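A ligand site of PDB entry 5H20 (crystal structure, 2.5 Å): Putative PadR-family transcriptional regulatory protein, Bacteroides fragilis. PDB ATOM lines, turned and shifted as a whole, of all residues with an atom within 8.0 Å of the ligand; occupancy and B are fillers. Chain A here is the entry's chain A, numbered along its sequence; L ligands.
The backbone NH (N) of Ser 31 sits at hydrogen-bond distance from an oxygen (O2) of the ligand, at 2.8 Å.
An oxygen (O3) of the ligand is in hydrogen-bond range of the backbone carbonyl oxygen (O) of Lys 76, 2.7 Å away.
O2 of the ligand lies within hydrogen-bond range of OG of Ser 31 (2.9 Å).
An oxygen (O1) of the ligand lies within hydrogen-bond range of the guanidinium group (NH2) of Arg 75.
N of Ala 30 sits at hydrogen-bond distance from O3 of the ligand (2.9 Å).
The side-chain hydroxyl (OH) of Tyr 50 is in hydrogen-bond range of the side-chain carboxylate (OE2) of Glu 46, 3.0 Å away.
The side-chain hydroxyl (OG) of Ser 31 sits at hydrogen-bond distance from the guanidinium group (NH2) of Arg 75.
The side-chain carboxylate (OD2) of Asp 32 lies within hydrogen-bond range of the backbone NH (N) of Tyr 29 (2.9 Å).
The backbone carbonyl oxygen (O) of Tyr 50 lies within hydrogen-bond range of the side-chain hydroxyl (OG1) of Thr 54 (3.2 Å).
The backbone carbonyl oxygen (O) of Arg 75 is in hydrogen-bond range of the backbone NH (N) of Val 67 (2.8 Å).
The side-chain amino group (NZ) of Lys 76 lies within hydrogen-bond range of the side-chain hydroxyl (OH) of Tyr 64 (3.0 Å).
O of Tyr 78 is in hydrogen-bond range of N of Ala 28, 2.9 Å away.
Tyr 29 touches the ligand.
OH of Tyr 50 touches O5 of the ligand, at 3.9 Å.
Pro 74 touches the ligand (O to C6, 3.6 Å).
Tyr 78 touches the ligand.
Hydrophobic or aromatic side chains within 4 Å of the ligand: Tyr 29, Ala 30 and Tyr 78.
Of the 22 residues printed, 8 come within 4 Å of the ligand.
The nearest printed residue that does not touch the ligand is Trp 66 (4.4 Å).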
ATOM      1  N   ALA A  28      24.148 -25.122   0.774  1.00  0.00           N
ATOM      2  CA  ALA A  28      25.205 -26.123   0.936  1.00  0.00           C
ATOM      3  C   ALA A  28      25.866 -26.563  -0.367  1.00  0.00           C
ATOM      4  O   ALA A  28      25.233 -26.531  -1.425  1.00  0.00           O
ATOM      5  CB  ALA A  28      24.661 -27.345   1.675  1.00  0.00           C
ATOM      6  N   TYR A  29      27.137 -26.949  -0.254  1.00  0.00           N
ATOM      7  CA  TYR A  29      27.836 -27.678  -1.299  1.00  0.00           C
ATOM      8  C   TYR A  29      27.297 -29.108  -1.299  1.00  0.00           C
ATOM      9  O   TYR A  29      26.815 -29.612  -0.266  1.00  0.00           O
ATOM     10  CB  TYR A  29      29.353 -27.709  -1.042  1.00  0.00           C
ATOM     11  CG  TYR A  29      30.060 -26.350  -0.948  1.00  0.00           C
ATOM     12  CD1 TYR A  29      30.290 -25.562  -2.083  1.00  0.00           C
ATOM     13  CD2 TYR A  29      30.525 -25.867   0.285  1.00  0.00           C
ATOM     14  CE1 TYR A  29      30.941 -24.336  -2.000  1.00  0.00           C
ATOM     15  CE2 TYR A  29      31.174 -24.641   0.377  1.00  0.00           C
ATOM     16  CZ  TYR A  29      31.380 -23.880  -0.760  1.00  0.00           C
ATOM     17  OH  TYR A  29      32.017 -22.673  -0.669  1.00  0.00           O
ATOM     18  N   ALA A  30      27.350 -29.762  -2.462  1.00  0.00           N
ATOM     19  CA  ALA A  30      27.027 -31.185  -2.577  1.00  0.00           C
ATOM     20  C   ALA A  30      27.697 -32.060  -1.493  1.00  0.00           C
ATOM     21  O   ALA A  30      27.046 -32.940  -0.925  1.00  0.00           O
ATOM     22  CB  ALA A  30      27.368 -31.695  -3.972  1.00  0.00           C
ATOM     23  N   SER A  31      28.975 -31.795  -1.224  1.00  0.00           N
ATOM     24  CA  SER A  31      29.738 -32.408  -0.120  1.00  0.00           C
ATOM     25  C   SER A  31      29.144 -32.177   1.278  1.00  0.00           C
ATOM     26  O   SER A  31      29.333 -33.022   2.154  1.00  0.00           O
ATOM     27  CB  SER A  31      31.190 -31.925  -0.139  1.00  0.00           C
ATOM     28  OG  SER A  31      31.245 -30.498  -0.131  1.00  0.00           O
ATOM     29  N   ASP A  32      28.456 -31.053   1.488  1.00  0.00           N
ATOM     30  CA  ASP A  32      27.760 -30.831   2.767  1.00  0.00           C
ATOM     31  C   ASP A  32      26.522 -31.707   2.846  1.00  0.00           C
ATOM     32  O   ASP A  32      26.206 -32.222   3.920  1.00  0.00           O
ATOM     33  CB  ASP A  32      27.365 -29.355   2.978  1.00  0.00           C
ATOM     34  CG  ASP A  32      28.540 -28.410   2.904  1.00  0.00           C
ATOM     35  OD1 ASP A  32      29.611 -28.742   3.476  1.00  0.00           O
ATOM     36  OD2 ASP A  32      28.397 -27.310   2.296  1.00  0.00           O
ATOM     37  N   ILE A  33      25.829 -31.841   1.716  1.00  0.00           N
ATOM     38  CA  ILE A  33      24.640 -32.679   1.609  1.00  0.00           C
ATOM     39  C   ILE A  33      25.011 -34.146   1.871  1.00  0.00           C
ATOM     40  O   ILE A  33      24.382 -34.787   2.714  1.00  0.00           O
ATOM     41  CB  ILE A  33      23.905 -32.522   0.241  1.00  0.00           C
ATOM     42  CG1 ILE A  33      23.302 -31.118   0.134  1.00  0.00           C
ATOM     43  CG2 ILE A  33      22.810 -33.577   0.081  1.00  0.00           C
ATOM     44  CD1 ILE A  33      22.916 -30.708  -1.269  1.00  0.00           C
ATOM     45  N   ILE A  34      26.057 -34.618   1.187  1.00  0.00           N
ATOM     46  CA  ILE A  34      26.602 -35.971   1.372  1.00  0.00           C
ATOM     47  C   ILE A  34      26.946 -36.211   2.849  1.00  0.00           C
ATOM     48  O   ILE A  34      26.593 -37.264   3.398  1.00  0.00           O
ATOM     49  CB  ILE A  34      27.812 -36.263   0.431  1.00  0.00           C
ATOM     50  CG1 ILE A  34      27.354 -36.320  -1.039  1.00  0.00           C
ATOM     51  CG2 ILE A  34      28.563 -37.557   0.821  1.00  0.00           C
ATOM     52  CD1 ILE A  34      28.460 -36.055  -2.071  1.00  0.00           C
ATOM     53  N   GLU A  46      28.232 -39.576  -5.189  1.00  0.00           N
ATOM     54  CA  GLU A  46      28.219 -38.507  -6.189  1.00  0.00           C
ATOM     55  C   GLU A  46      27.432 -38.895  -7.443  1.00  0.00           C
ATOM     56  O   GLU A  46      26.604 -38.129  -7.907  1.00  0.00           O
ATOM     57  CB  GLU A  46      29.644 -38.071  -6.545  1.00  0.00           C
ATOM     58  CG  GLU A  46      30.433 -37.485  -5.385  1.00  0.00           C
ATOM     59  CD  GLU A  46      31.852 -37.018  -5.744  1.00  0.00           C
ATOM     60  OE1 GLU A  46      32.420 -37.466  -6.767  1.00  0.00           O
ATOM     61  OE2 GLU A  46      32.405 -36.200  -4.973  1.00  0.00           O
ATOM     62  N   LEU A  49      23.770 -38.507  -6.306  1.00  0.00           N
ATOM     63  CA  LEU A  49      23.413 -37.150  -5.888  1.00  0.00           C
ATOM     64  C   LEU A  49      23.462 -36.115  -7.029  1.00  0.00           C
ATOM     65  O   LEU A  49      22.532 -35.334  -7.206  1.00  0.00           O
ATOM     66  CB  LEU A  49      24.318 -36.700  -4.730  1.00  0.00           C
ATOM     67  CG  LEU A  49      23.922 -35.698  -3.627  1.00  0.00           C
ATOM     68  CD1 LEU A  49      24.975 -34.618  -3.497  1.00  0.00           C
ATOM     69  CD2 LEU A  49      22.554 -35.049  -3.803  1.00  0.00           C
ATOM     70  N   TYR A  50      24.556 -36.122  -7.803  1.00  0.00           N
ATOM     71  CA  TYR A  50      24.818 -35.092  -8.824  1.00  0.00           C
ATOM     72  C   TYR A  50      23.699 -34.922  -9.874  1.00  0.00           C
ATOM     73  O   TYR A  50      23.279 -33.780 -10.106  1.00  0.00           O
ATOM     74  CB  TYR A  50      26.205 -35.257  -9.467  1.00  0.00           C
ATOM     75  CG  TYR A  50      27.398 -34.918  -8.567  1.00  0.00           C
ATOM     76  CD1 TYR A  50      27.229 -34.625  -7.200  1.00  0.00           C
ATOM     77  CD2 TYR A  50      28.702 -34.915  -9.081  1.00  0.00           C
ATOM     78  CE1 TYR A  50      28.310 -34.313  -6.379  1.00  0.00           C
ATOM     79  CE2 TYR A  50      29.793 -34.615  -8.268  1.00  0.00           C
ATOM     80  CZ  TYR A  50      29.586 -34.318  -6.918  1.00  0.00           C
ATOM     81  OH  TYR A  50      30.641 -34.022  -6.080  1.00  0.00           O
ATOM     82  N   LEU A  53      20.537 -33.151  -8.222  1.00  0.00           N
ATOM     83  CA  LEU A  53      20.818 -31.740  -8.052  1.00  0.00           C
ATOM     84  C   LEU A  53      20.605 -30.988  -9.374  1.00  0.00           C
ATOM     85  O   LEU A  53      19.917 -29.963  -9.402  1.00  0.00           O
ATOM     86  CB  LEU A  53      22.251 -31.528  -7.550  1.00  0.00           C
ATOM     87  CG  LEU A  53      22.654 -32.124  -6.204  1.00  0.00           C
ATOM     88  CD1 LEU A  53      24.144 -31.880  -5.989  1.00  0.00           C
ATOM     89  CD2 LEU A  53      21.818 -31.535  -5.073  1.00  0.00           C
ATOM     90  N   THR A  54      21.189 -31.541 -10.450  1.00  0.00           N
ATOM     91  CA  THR A  54      21.066 -31.014 -11.804  1.00  0.00           C
ATOM     92  C   THR A  54      19.592 -30.985 -12.246  1.00  0.00           C
ATOM     93  O   THR A  54      19.141 -29.951 -12.782  1.00  0.00           O
ATOM     94  CB  THR A  54      21.997 -31.774 -12.796  1.00  0.00           C
ATOM     95  OG1 THR A  54      23.363 -31.558 -12.428  1.00  0.00           O
ATOM     96  CG2 THR A  54      21.822 -31.305 -14.248  1.00  0.00           C
ATOM     97  N   TYR A  64      22.201 -22.293  -8.009  1.00  0.00           N
ATOM     98  CA  TYR A  64      23.539 -22.259  -7.452  1.00  0.00           C
ATOM     99  C   TYR A  64      24.341 -21.043  -7.922  1.00  0.00           C
ATOM    100  O   TYR A  64      24.006 -20.374  -8.915  1.00  0.00           O
ATOM    101  CB  TYR A  64      24.301 -23.586  -7.709  1.00  0.00           C
ATOM    102  CG  TYR A  64      24.654 -23.836  -9.148  1.00  0.00           C
ATOM    103  CD1 TYR A  64      25.759 -23.203  -9.744  1.00  0.00           C
ATOM    104  CD2 TYR A  64      23.893 -24.697  -9.932  1.00  0.00           C
ATOM    105  CE1 TYR A  64      26.086 -23.425 -11.077  1.00  0.00           C
ATOM    106  CE2 TYR A  64      24.208 -24.928 -11.266  1.00  0.00           C
ATOM    107  CZ  TYR A  64      25.299 -24.281 -11.825  1.00  0.00           C
ATOM    108  OH  TYR A  64      25.590 -24.529 -13.153  1.00  0.00           O
ATOM    109  N   GLU A  65      25.410 -20.773  -7.182  1.00  0.00           N
ATOM    110  CA  GLU A  65      26.448 -19.830  -7.574  1.00  0.00           C
ATOM    111  C   GLU A  65      27.797 -20.518  -7.431  1.00  0.00           C
ATOM    112  O   GLU A  65      27.975 -21.403  -6.585  1.00  0.00           O
ATOM    113  CB  GLU A  65      26.356 -18.517  -6.783  1.00  0.00           C
ATOM    114  CG  GLU A  65      25.657 -18.595  -5.426  1.00  0.00           C
ATOM    115  CD  GLU A  65      25.057 -17.283  -4.947  1.00  0.00           C
ATOM    116  OE1 GLU A  65      25.403 -16.187  -5.480  1.00  0.00           O
ATOM    117  OE2 GLU A  65      24.214 -17.346  -4.023  1.00  0.00           O
ATOM    118  N   TRP A  66      28.731 -20.163  -8.305  1.00  0.00           N
ATOM    119  CA  TRP A  66      30.087 -20.715  -8.270  1.00  0.00           C
ATOM    120  C   TRP A  66      30.916 -20.015  -7.190  1.00  0.00           C
ATOM    121  O   TRP A  66      30.945 -18.785  -7.125  1.00  0.00           O
ATOM    122  CB  TRP A  66      30.755 -20.562  -9.626  1.00  0.00           C
ATOM    123  CG  TRP A  66      30.131 -21.361 -10.726  1.00  0.00           C
ATOM    124  CD1 TRP A  66      29.232 -20.914 -11.651  1.00  0.00           C
ATOM    125  CD2 TRP A  66      30.359 -22.747 -11.021  1.00  0.00           C
ATOM    126  NE1 TRP A  66      28.894 -21.926 -12.505  1.00  0.00           N
ATOM    127  CE2 TRP A  66      29.567 -23.068 -12.137  1.00  0.00           C
ATOM    128  CE3 TRP A  66      31.155 -23.747 -10.437  1.00  0.00           C
ATOM    129  CZ2 TRP A  66      29.551 -24.359 -12.715  1.00  0.00           C
ATOM    130  CZ3 TRP A  66      31.148 -25.038 -11.003  1.00  0.00           C
ATOM    131  CH2 TRP A  66      30.353 -25.320 -12.132  1.00  0.00           C
ATOM    132  N   VAL A  67      31.566 -20.814  -6.338  1.00  0.00           N
ATOM    133  CA  VAL A  67      32.533 -20.320  -5.374  1.00  0.00           C
ATOM    134  C   VAL A  67      33.896 -20.512  -6.020  1.00  0.00           C
ATOM    135  O   VAL A  67      34.335 -21.643  -6.273  1.00  0.00           O
ATOM    136  CB  VAL A  67      32.401 -21.043  -4.003  1.00  0.00           C
ATOM    137  CG1 VAL A  67      33.532 -20.643  -3.056  1.00  0.00           C
ATOM    138  CG2 VAL A  67      31.053 -20.731  -3.351  1.00  0.00           C
ATOM    139  N   PRO A  73      39.250 -26.060  -7.270  1.00  0.00           N
ATOM    140  CA  PRO A  73      38.365 -25.794  -8.407  1.00  0.00           C
ATOM    141  C   PRO A  73      37.115 -24.999  -8.000  1.00  0.00           C
ATOM    142  O   PRO A  73      36.863 -24.852  -6.792  1.00  0.00           O
ATOM    143  CB  PRO A  73      37.974 -27.210  -8.870  1.00  0.00           C
ATOM    144  CG  PRO A  73      37.988 -27.997  -7.611  1.00  0.00           C
ATOM    145  CD  PRO A  73      39.192 -27.483  -6.872  1.00  0.00           C
ATOM    146  N   PRO A  74      36.349 -24.482  -8.988  1.00  0.00           N
ATOM    147  CA  PRO A  74      35.051 -23.855  -8.662  1.00  0.00           C
ATOM    148  C   PRO A  74      34.037 -24.857  -8.109  1.00  0.00           C
ATOM    149  O   PRO A  74      33.905 -25.968  -8.647  1.00  0.00           O
ATOM    150  CB  PRO A  74      34.558 -23.318 -10.010  1.00  0.00           C
ATOM    151  CG  PRO A  74      35.808 -23.126 -10.820  1.00  0.00           C
ATOM    152  CD  PRO A  74      36.721 -24.239 -10.402  1.00  0.00           C
ATOM    153  N   ARG A  75      33.350 -24.472  -7.042  1.00  0.00           N
ATOM    154  CA  ARG A  75      32.402 -25.347  -6.363  1.00  0.00           C
ATOM    155  C   ARG A  75      31.006 -24.741  -6.470  1.00  0.00           C
ATOM    156  O   ARG A  75      30.853 -23.514  -6.365  1.00  0.00           O
ATOM    157  CB  ARG A  75      32.797 -25.533  -4.900  1.00  0.00           C
ATOM    158  CG  ARG A  75      34.202 -26.086  -4.683  1.00  0.00           C
ATOM    159  CD  ARG A  75      34.540 -26.143  -3.208  1.00  0.00           C
ATOM    160  NE  ARG A  75      33.844 -27.246  -2.563  1.00  0.00           N
ATOM    161  CZ  ARG A  75      33.536 -27.330  -1.269  1.00  0.00           C
ATOM    162  NH1 ARG A  75      33.860 -26.346  -0.416  1.00  0.00           N
ATOM    163  NH2 ARG A  75      32.880 -28.395  -0.813  1.00  0.00           N
ATOM    164  N   LYS A  76      30.016 -25.582  -6.715  1.00  0.00           N
ATOM    165  CA  LYS A  76      28.617 -25.158  -6.832  1.00  0.00           C
ATOM    166  C   LYS A  76      28.041 -25.019  -5.426  1.00  0.00           C
ATOM    167  O   LYS A  76      28.139 -25.914  -4.593  1.00  0.00           O
ATOM    168  CB  LYS A  76      27.798 -26.144  -7.670  1.00  0.00           C
ATOM    169  CG  LYS A  76      28.047 -26.109  -9.174  1.00  0.00           C
ATOM    170  CD  LYS A  76      27.343 -27.286  -9.828  1.00  0.00           C
ATOM    171  CE  LYS A  76      27.660 -27.412 -11.321  1.00  0.00           C
ATOM    172  NZ  LYS A  76      26.470 -27.235 -12.200  1.00  0.00           N
ATOM    173  N   TYR A  77      27.469 -23.849  -5.147  1.00  0.00           N
ATOM    174  CA  TYR A  77      26.912 -23.605  -3.825  1.00  0.00           C
ATOM    175  C   TYR A  77      25.418 -23.433  -3.994  1.00  0.00           C
ATOM    176  O   TYR A  77      24.936 -22.466  -4.583  1.00  0.00           O
ATOM    177  CB  TYR A  77      27.620 -22.438  -3.149  1.00  0.00           C
ATOM    178  CG  TYR A  77      27.327 -22.235  -1.677  1.00  0.00           C
ATOM    179  CD1 TYR A  77      27.788 -23.135  -0.700  1.00  0.00           C
ATOM    180  CD2 TYR A  77      26.609 -21.100  -1.239  1.00  0.00           C
ATOM    181  CE1 TYR A  77      27.540 -22.923   0.648  1.00  0.00           C
ATOM    182  CE2 TYR A  77      26.351 -20.886   0.107  1.00  0.00           C
ATOM    183  CZ  TYR A  77      26.807 -21.797   1.043  1.00  0.00           C
ATOM    184  OH  TYR A  77      26.548 -21.603   2.380  1.00  0.00           O
ATOM    185  N   TYR A  78      24.692 -24.425  -3.493  1.00  0.00           N
ATOM    186  CA  TYR A  78      23.289 -24.625  -3.818  1.00  0.00           C
ATOM    187  C   TYR A  78      22.408 -24.061  -2.734  1.00  0.00           C
ATOM    188  O   TYR A  78      22.720 -24.164  -1.545  1.00  0.00           O
ATOM    189  CB  TYR A  78      22.998 -26.124  -3.934  1.00  0.00           C
ATOM    190  CG  TYR A  78      23.514 -26.854  -5.163  1.00  0.00           C
ATOM    191  CD1 TYR A  78      22.756 -26.920  -6.339  1.00  0.00           C
ATOM    192  CD2 TYR A  78      24.734 -27.558  -5.112  1.00  0.00           C
ATOM    193  CE1 TYR A  78      23.205 -27.617  -7.450  1.00  0.00           C
ATOM    194  CE2 TYR A  78      25.190 -28.266  -6.221  1.00  0.00           C
ATOM    195  CZ  TYR A  78      24.424 -28.300  -7.380  1.00  0.00           C
ATOM    196  OH  TYR A  78      24.848 -29.013  -8.484  1.00  0.00           O
HETATM  197  C1  LIG L   1      32.286 -29.723  -4.540  1.00  0.00           C
HETATM  198  C2  LIG L   1      30.894 -29.369  -4.011  1.00  0.00           C
HETATM  199  C3  LIG L   1      29.773 -29.441  -5.057  1.00  0.00           C
HETATM  200  C4  LIG L   1      30.204 -29.197  -6.511  1.00  0.00           C
HETATM  201  C5  LIG L   1      31.500 -29.937  -6.902  1.00  0.00           C
HETATM  202  C6  LIG L   1      32.367 -29.059  -7.809  1.00  0.00           C
HETATM  203  O1  LIG L   1      32.964 -30.490  -3.533  1.00  0.00           O
HETATM  204  O2  LIG L   1      30.558 -30.266  -2.939  1.00  0.00           O
HETATM  205  O3  LIG L   1      28.749 -28.498  -4.711  1.00  0.00           O
HETATM  206  O4  LIG L   1      29.155 -29.647  -7.380  1.00  0.00           O
HETATM  207  O5  LIG L   1      32.239 -30.466  -5.776  1.00  0.00           O
HETATM  208  O6  LIG L   1      31.792 -29.013  -9.122  1.00  0.00           O
